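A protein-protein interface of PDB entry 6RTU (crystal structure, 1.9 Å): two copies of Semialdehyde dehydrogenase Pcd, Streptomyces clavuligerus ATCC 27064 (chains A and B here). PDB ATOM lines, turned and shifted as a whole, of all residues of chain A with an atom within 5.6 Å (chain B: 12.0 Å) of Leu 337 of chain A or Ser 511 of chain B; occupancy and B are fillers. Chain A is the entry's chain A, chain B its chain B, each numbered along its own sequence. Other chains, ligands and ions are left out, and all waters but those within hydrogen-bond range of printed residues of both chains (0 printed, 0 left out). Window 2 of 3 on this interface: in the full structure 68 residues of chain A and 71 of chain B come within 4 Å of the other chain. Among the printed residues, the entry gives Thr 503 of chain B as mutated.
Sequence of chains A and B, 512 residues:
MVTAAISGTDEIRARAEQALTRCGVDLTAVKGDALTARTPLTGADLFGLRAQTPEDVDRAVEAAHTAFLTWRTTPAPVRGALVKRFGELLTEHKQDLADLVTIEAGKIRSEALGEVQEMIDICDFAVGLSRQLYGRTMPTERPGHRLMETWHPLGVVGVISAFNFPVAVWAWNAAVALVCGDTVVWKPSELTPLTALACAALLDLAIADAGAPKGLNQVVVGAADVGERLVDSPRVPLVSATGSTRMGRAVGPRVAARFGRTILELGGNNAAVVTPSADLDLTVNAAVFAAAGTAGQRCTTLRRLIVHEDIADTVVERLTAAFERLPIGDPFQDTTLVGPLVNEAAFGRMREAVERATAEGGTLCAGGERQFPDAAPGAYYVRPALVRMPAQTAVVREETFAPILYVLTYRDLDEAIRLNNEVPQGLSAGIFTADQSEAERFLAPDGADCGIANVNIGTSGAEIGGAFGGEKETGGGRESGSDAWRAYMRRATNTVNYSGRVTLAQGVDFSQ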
ATOM      1  N   ILE A 108       1.359   9.033 -11.108  1.00  0.00           N
ATOM      2  CA  ILE A 108       2.164   9.507  -9.994  1.00  0.00           C
ATOM      3  C   ILE A 108       2.264   8.431  -8.918  1.00  0.00           C
ATOM      4  O   ILE A 108       1.477   7.479  -8.868  1.00  0.00           O
ATOM      5  CB  ILE A 108       1.612  10.824  -9.420  1.00  0.00           C
ATOM      6  CG1 ILE A 108       0.282  10.600  -8.684  1.00  0.00           C
ATOM      7  CG2 ILE A 108       1.481  11.863 -10.538  1.00  0.00           C
ATOM      8  CD1 ILE A 108      -0.258  11.874  -8.027  1.00  0.00           C
ATOM      9  N   GLU A 111      -0.803   7.374  -6.818  1.00  0.00           N
ATOM     10  CA  GLU A 111      -1.833   6.625  -7.536  1.00  0.00           C
ATOM     11  C   GLU A 111      -1.357   5.226  -7.908  1.00  0.00           C
ATOM     12  O   GLU A 111      -2.164   4.292  -7.924  1.00  0.00           O
ATOM     13  CB  GLU A 111      -2.304   7.377  -8.792  1.00  0.00           C
ATOM     14  CG  GLU A 111      -3.144   8.648  -8.516  1.00  0.00           C
ATOM     15  CD  GLU A 111      -3.838   9.188  -9.778  1.00  0.00           C
ATOM     16  OE1 GLU A 111      -4.629   8.443 -10.403  1.00  0.00           O
ATOM     17  OE2 GLU A 111      -3.581  10.348 -10.165  1.00  0.00           O
ATOM     18  N   ALA A 292      -8.598  15.483 -13.007  1.00  0.00           N
ATOM     19  CA  ALA A 292      -7.179  15.545 -13.350  1.00  0.00           C
ATOM     20  C   ALA A 292      -6.391  14.305 -12.951  1.00  0.00           C
ATOM     21  O   ALA A 292      -5.301  14.096 -13.496  1.00  0.00           O
ATOM     22  CB  ALA A 292      -6.517  16.776 -12.700  1.00  0.00           C
ATOM     23  N   GLY A 293      -6.895  13.505 -12.010  1.00  0.00           N
ATOM     24  CA  GLY A 293      -6.168  12.315 -11.599  1.00  0.00           C
ATOM     25  C   GLY A 293      -5.913  11.394 -12.780  1.00  0.00           C
ATOM     26  O   GLY A 293      -6.735  11.273 -13.693  1.00  0.00           O
ATOM     27  N   THR A 294      -4.739  10.763 -12.774  1.00  0.00           N
ATOM     28  CA  THR A 294      -4.322   9.878 -13.863  1.00  0.00           C
ATOM     29  C   THR A 294      -4.289  10.632 -15.195  1.00  0.00           C
ATOM     30  O   THR A 294      -4.489  10.045 -16.258  1.00  0.00           O
ATOM     31  CB  THR A 294      -5.238   8.649 -13.947  1.00  0.00           C
ATOM     32  OG1 THR A 294      -5.635   8.285 -12.620  1.00  0.00           O
ATOM     33  CG2 THR A 294      -4.525   7.454 -14.608  1.00  0.00           C
ATOM     34  N   LEU A 326      -1.967  23.360 -10.660  1.00  0.00           N
ATOM     35  CA  LEU A 326      -1.611  21.946 -10.633  1.00  0.00           C
ATOM     36  C   LEU A 326      -0.148  21.763 -11.016  1.00  0.00           C
ATOM     37  O   LEU A 326       0.279  22.264 -12.064  1.00  0.00           O
ATOM     38  CB  LEU A 326      -2.493  21.138 -11.588  1.00  0.00           C
ATOM     39  CG  LEU A 326      -3.903  20.830 -11.072  1.00  0.00           C
ATOM     40  CD1 LEU A 326      -4.738  20.149 -12.144  1.00  0.00           C
ATOM     41  CD2 LEU A 326      -3.825  19.968  -9.833  1.00  0.00           C
ATOM     42  N   PRO A 327       0.639  21.042 -10.217  1.00  0.00           N
ATOM     43  CA  PRO A 327       2.042  20.772 -10.576  1.00  0.00           C
ATOM     44  C   PRO A 327       2.133  19.611 -11.560  1.00  0.00           C
ATOM     45  O   PRO A 327       1.776  18.476 -11.241  1.00  0.00           O
ATOM     46  CB  PRO A 327       2.690  20.429  -9.229  1.00  0.00           C
ATOM     47  CG  PRO A 327       1.564  19.889  -8.403  1.00  0.00           C
ATOM     48  CD  PRO A 327       0.295  20.555  -8.872  1.00  0.00           C
ATOM     49  N   ILE A 328       2.603  19.906 -12.763  1.00  0.00           N
ATOM     50  CA  ILE A 328       2.775  18.922 -13.825  1.00  0.00           C
ATOM     51  C   ILE A 328       4.257  18.587 -13.918  1.00  0.00           C
ATOM     52  O   ILE A 328       5.105  19.483 -13.833  1.00  0.00           O
ATOM     53  CB  ILE A 328       2.227  19.488 -15.150  1.00  0.00           C
ATOM     54  CG1 ILE A 328       0.773  19.920 -14.940  1.00  0.00           C
ATOM     55  CG2 ILE A 328       2.336  18.492 -16.276  1.00  0.00           C
ATOM     56  CD1 ILE A 328       0.355  21.011 -15.839  1.00  0.00           C
ATOM     57  N   THR A 335       6.472  15.965  -5.721  1.00  0.00           N
ATOM     58  CA  THR A 335       5.733  17.203  -5.957  1.00  0.00           C
ATOM     59  C   THR A 335       4.692  17.078  -7.072  1.00  0.00           C
ATOM     60  O   THR A 335       3.743  17.864  -7.105  1.00  0.00           O
ATOM     61  CB  THR A 335       6.716  18.326  -6.299  1.00  0.00           C
ATOM     62  OG1 THR A 335       7.577  17.887  -7.361  1.00  0.00           O
ATOM     63  CG2 THR A 335       7.572  18.664  -5.098  1.00  0.00           C
ATOM     64  N   THR A 336       4.843  16.119  -7.986  1.00  0.00           N
ATOM     65  CA  THR A 336       3.967  16.054  -9.146  1.00  0.00           C
ATOM     66  C   THR A 336       2.571  15.534  -8.790  1.00  0.00           C
ATOM     67  O   THR A 336       2.422  14.542  -8.069  1.00  0.00           O
ATOM     68  CB  THR A 336       4.594  15.160 -10.216  1.00  0.00           C
ATOM     69  OG1 THR A 336       5.866  15.696 -10.601  1.00  0.00           O
ATOM     70  CG2 THR A 336       3.694  15.068 -11.447  1.00  0.00           C
ATOM     71  N   LEU A 337       1.541  16.198  -9.326  1.00  0.00           N
ATOM     72  CA  LEU A 337       0.179  15.669  -9.321  1.00  0.00           C
ATOM     73  C   LEU A 337      -0.316  15.228 -10.693  1.00  0.00           C
ATOM     74  O   LEU A 337      -1.255  14.427 -10.758  1.00  0.00           O
ATOM     75  CB  LEU A 337      -0.814  16.706  -8.763  1.00  0.00           C
ATOM     76  CG  LEU A 337      -0.658  16.988  -7.261  1.00  0.00           C
ATOM     77  CD1 LEU A 337      -1.694  18.022  -6.797  1.00  0.00           C
ATOM     78  CD2 LEU A 337      -0.759  15.699  -6.445  1.00  0.00           C
ATOM     79  N   VAL A 338       0.279  15.716 -11.785  1.00  0.00           N
ATOM     80  CA  VAL A 338      -0.147  15.360 -13.142  1.00  0.00           C
ATOM     81  C   VAL A 338       1.081  14.901 -13.920  1.00  0.00           C
ATOM     82  O   VAL A 338       1.992  15.702 -14.170  1.00  0.00           O
ATOM     83  CB  VAL A 338      -0.836  16.520 -13.879  1.00  0.00           C
ATOM     84  CG1 VAL A 338      -1.301  16.064 -15.287  1.00  0.00           C
ATOM     85  CG2 VAL A 338      -1.996  17.092 -13.075  1.00  0.00           C
ATOM     86  N   GLY A 339       1.104  13.619 -14.304  1.00  0.00           N
ATOM     87  CA  GLY A 339       2.104  13.089 -15.215  1.00  0.00           C
ATOM     88  C   GLY A 339       1.649  13.180 -16.662  1.00  0.00           C
ATOM     89  O   GLY A 339       0.680  13.868 -16.976  1.00  0.00           O
ATOM     90  N   ARG B 501     -15.543  16.195   4.247  1.00  0.00           N
ATOM     91  CA  ARG B 501     -14.174  16.241   3.759  1.00  0.00           C
ATOM     92  C   ARG B 501     -14.028  15.251   2.610  1.00  0.00           C
ATOM     93  O   ARG B 501     -14.837  14.336   2.453  1.00  0.00           O
ATOM     94  CB  ARG B 501     -13.170  15.944   4.891  1.00  0.00           C
ATOM     95  CG  ARG B 501     -12.959  14.468   5.179  1.00  0.00           C
ATOM     96  CD  ARG B 501     -12.035  14.247   6.391  1.00  0.00           C
ATOM     97  NE  ARG B 501     -12.673  14.645   7.647  1.00  0.00           N
ATOM     98  CZ  ARG B 501     -13.382  13.829   8.428  1.00  0.00           C
ATOM     99  NH1 ARG B 501     -13.541  12.548   8.098  1.00  0.00           N
ATOM    100  NH2 ARG B 501     -13.931  14.293   9.548  1.00  0.00           N
ATOM    101  N   VAL B 502     -13.005  15.466   1.783  1.00  0.00           N
ATOM    102  CA  VAL B 502     -12.659  14.537   0.711  1.00  0.00           C
ATOM    103  C   VAL B 502     -11.693  13.508   1.287  1.00  0.00           C
ATOM    104  O   VAL B 502     -10.594  13.857   1.737  1.00  0.00           O
ATOM    105  CB  VAL B 502     -12.039  15.261  -0.497  1.00  0.00           C
ATOM    106  CG1 VAL B 502     -11.646  14.234  -1.602  1.00  0.00           C
ATOM    107  CG2 VAL B 502     -12.978  16.347  -1.065  1.00  0.00           C
ATOM    108  N   THR B 503     -12.114  12.248   1.304  1.00  0.00           N
ATOM    109  CA  THR B 503     -11.262  11.120   1.667  1.00  0.00           C
ATOM    110  C   THR B 503     -11.198  10.168   0.480  1.00  0.00           C
ATOM    111  O   THR B 503     -12.238   9.702   0.002  1.00  0.00           O
ATOM    112  CB  THR B 503     -11.803  10.408   2.909  1.00  0.00           C
ATOM    113  OG1 THR B 503     -11.701  11.287   4.038  1.00  0.00           O
ATOM    114  CG2 THR B 503     -11.021   9.116   3.183  1.00  0.00           C
ATOM    115  N   LEU B 504      -9.990   9.894  -0.010  1.00  0.00           N
ATOM    116  CA  LEU B 504      -9.823   9.050  -1.190  1.00  0.00           C
ATOM    117  C   LEU B 504      -9.539   7.606  -0.786  1.00  0.00           C
ATOM    118  O   LEU B 504      -8.841   7.350   0.202  1.00  0.00           O
ATOM    119  CB  LEU B 504      -8.699   9.582  -2.085  1.00  0.00           C
ATOM    120  CG  LEU B 504      -8.849  11.031  -2.564  1.00  0.00           C
ATOM    121  CD1 LEU B 504      -7.669  11.436  -3.479  1.00  0.00           C
ATOM    122  CD2 LEU B 504     -10.199  11.244  -3.264  1.00  0.00           C
ATOM    123  N   ALA B 505     -10.102   6.667  -1.547  1.00  0.00           N
ATOM    124  CA  ALA B 505      -9.890   5.248  -1.301  1.00  0.00           C
ATOM    125  C   ALA B 505      -8.425   4.868  -1.521  1.00  0.00           C
ATOM    126  O   ALA B 505      -7.672   5.567  -2.207  1.00  0.00           O
ATOM    127  CB  ALA B 505     -10.779   4.408  -2.222  1.00  0.00           C
ATOM    128  N   GLY B 507      -5.830   5.021   0.180  1.00  0.00           N
ATOM    129  CA  GLY B 507      -4.768   5.886   0.659  1.00  0.00           C
ATOM    130  C   GLY B 507      -4.171   6.796  -0.389  1.00  0.00           C
ATOM    131  O   GLY B 507      -3.033   7.253  -0.228  1.00  0.00           O
ATOM    132  N   VAL B 508      -4.892   7.055  -1.479  1.00  0.00           N
ATOM    133  CA  VAL B 508      -4.395   7.970  -2.496  1.00  0.00           C
ATOM    134  C   VAL B 508      -4.410   9.387  -1.935  1.00  0.00           C
ATOM    135  O   VAL B 508      -5.309   9.768  -1.167  1.00  0.00           O
ATOM    136  CB  VAL B 508      -5.225   7.860  -3.791  1.00  0.00           C
ATOM    137  CG1 VAL B 508      -4.804   8.925  -4.805  1.00  0.00           C
ATOM    138  CG2 VAL B 508      -5.073   6.472  -4.426  1.00  0.00           C
ATOM    139  N   ASP B 509      -3.402  10.171  -2.305  1.00  0.00           N
ATOM    140  CA  ASP B 509      -3.239  11.533  -1.823  1.00  0.00           C
ATOM    141  C   ASP B 509      -3.021  12.445  -3.020  1.00  0.00           C
ATOM    142  O   ASP B 509      -2.024  12.304  -3.739  1.00  0.00           O
ATOM    143  CB  ASP B 509      -2.070  11.620  -0.838  1.00  0.00           C
ATOM    144  CG  ASP B 509      -1.788  13.038  -0.382  1.00  0.00           C
ATOM    145  OD1 ASP B 509      -2.639  13.930  -0.606  1.00  0.00           O
ATOM    146  OD2 ASP B 509      -0.717  13.254   0.222  1.00  0.00           O
ATOM    147  N   PHE B 510      -3.947  13.377  -3.226  1.00  0.00           N
ATOM    148  CA  PHE B 510      -3.869  14.319  -4.336  1.00  0.00           C
ATOM    149  C   PHE B 510      -3.664  15.753  -3.851  1.00  0.00           C
ATOM    150  O   PHE B 510      -4.025  16.705  -4.545  1.00  0.00           O
ATOM    151  CB  PHE B 510      -5.114  14.219  -5.219  1.00  0.00           C
ATOM    152  CG  PHE B 510      -4.835  14.444  -6.677  1.00  0.00           C
ATOM    153  CD1 PHE B 510      -4.075  13.531  -7.400  1.00  0.00           C
ATOM    154  CD2 PHE B 510      -5.326  15.570  -7.325  1.00  0.00           C
ATOM    155  CE1 PHE B 510      -3.805  13.731  -8.733  1.00  0.00           C
ATOM    156  CE2 PHE B 510      -5.057  15.785  -8.666  1.00  0.00           C
ATOM    157  CZ  PHE B 510      -4.295  14.864  -9.375  1.00  0.00           C
ATOM    158  N   SER B 511      -3.048  15.913  -2.678  1.00  0.00           N
ATOM    159  CA  SER B 511      -2.740  17.219  -2.113  1.00  0.00           C
ATOM    160  C   SER B 511      -1.380  17.714  -2.593  1.00  0.00           C
ATOM    161  O   SER B 511      -0.497  16.929  -2.959  1.00  0.00           O
ATOM    162  CB  SER B 511      -2.749  17.157  -0.587  1.00  0.00           C
ATOM    163  OG  SER B 511      -1.615  16.438  -0.127  1.00  0.00           O
ATOM    164  N   GLN B 512      -1.213  19.032  -2.573  1.00  0.00           N
ATOM    165  CA  GLN B 512       0.020  19.651  -3.049  1.00  0.00           C
ATOM    166  C   GLN B 512       0.565  20.636  -2.021  1.00  0.00           C
ATOM    167  O   GLN B 512       0.007  20.775  -0.930  1.00  0.00           O
ATOM    168  CB  GLN B 512      -0.214  20.348  -4.393  1.00  0.00           C
ATOM    169  CG  GLN B 512      -1.124  21.570  -4.322  1.00  0.00           C
ATOM    170  CD  GLN B 512      -1.489  22.116  -5.697  1.00  0.00           C
ATOM    171  OE1 GLN B 512      -2.412  21.625  -6.366  1.00  0.00           O
ATOM    172  NE2 GLN B 512      -0.747  23.124  -6.135  1.00  0.00           N
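OE1 of Glu 111 of chain A sits at hydrogen-bond distance from OG1 of Thr 294 of chain A (2.4 Å). The backbone carbonyl oxygen (O) of Pro 327 of chain A is in hydrogen-bond range of the backbone NH (N) of Leu 337 of chain A, at 3.0 Å. The backbone NH (N) of Val 338 of chain A sits at hydrogen-bond distance from the backbone carbonyl oxygen (O) of Pro 327 of chain A. The side-chain carboxylate of Asp 509 of chain B is in hydrogen-bond range of the side-chain hydroxyl of Ser 511 of chain B, at 2.8 Å.
Among the printed residues, pairs that only touch across the chains: Leu 337 of chain A with Phe 510 of chain B, Leu 337 of chain A with Gln 512 of chain B, Glu 111 of chain A with Phe 510 of chain B, Leu 337 of chain A with Ser 511 of chain B, Pro 327 of chain A with Gln 512 of chain B and Gly 293 of chain A with Phe 510 of chain B.
No residue of chain B comes within 4 Å of Ile 108 of chain A. Of the printed residues of chain B, Glu 111 of chain A touches Phe 510. No residue of chain B comes within 4 Å of Ala 292 of chain A. Gly 293 of chain A touches just one residue of chain B: Phe 510. Leu 326 of chain A touches none of the printed residues of chain B. Pro 327 of chain A touches just one residue of chain B: Gln 512. No residue of chain B comes within 4 Å of Ile 328 of chain A. No residue of chain B comes within 4 Å of Thr 336 of chain A. No residue of chain B comes within 4 Å of Val 338 of chain A. No residue of chain B comes within 4 Å of Gly 339 of chain A. Thr 503 of chain B touches none of the printed residues of chain A. Of the printed residues of chain A, Phe 510 of chain B touches Glu 111 (3.7 Å), Gly 293 (3.9 Å) and Leu 337 (3.3 Å). Of chain A, only Leu 337 (3.7 Å) comes within 4 Å of Ser 511 of chain B. Of the printed residues of chain A, Gln 512 of chain B touches Pro 327 and Leu 337. The nearest printed residue of chain A that does not touch Ser 511 of chain B is Thr 335 of chain A (6.0 Å). The nearest printed residue of chain A that does not touch Phe 510 of chain B is Ile 108 of chain A (4.1 Å).
Printed residues of chain B that touch a printed residue of chain A: Phe 510, Ser 511 and Gln 512. Of the 13 printed residues of chain A, 4 touch a printed residue of chain B.
No position is printed for both chains. Of the 6 pairs that touch across the chains among the printed residues, none has its exchanged pair printed and touching as well.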
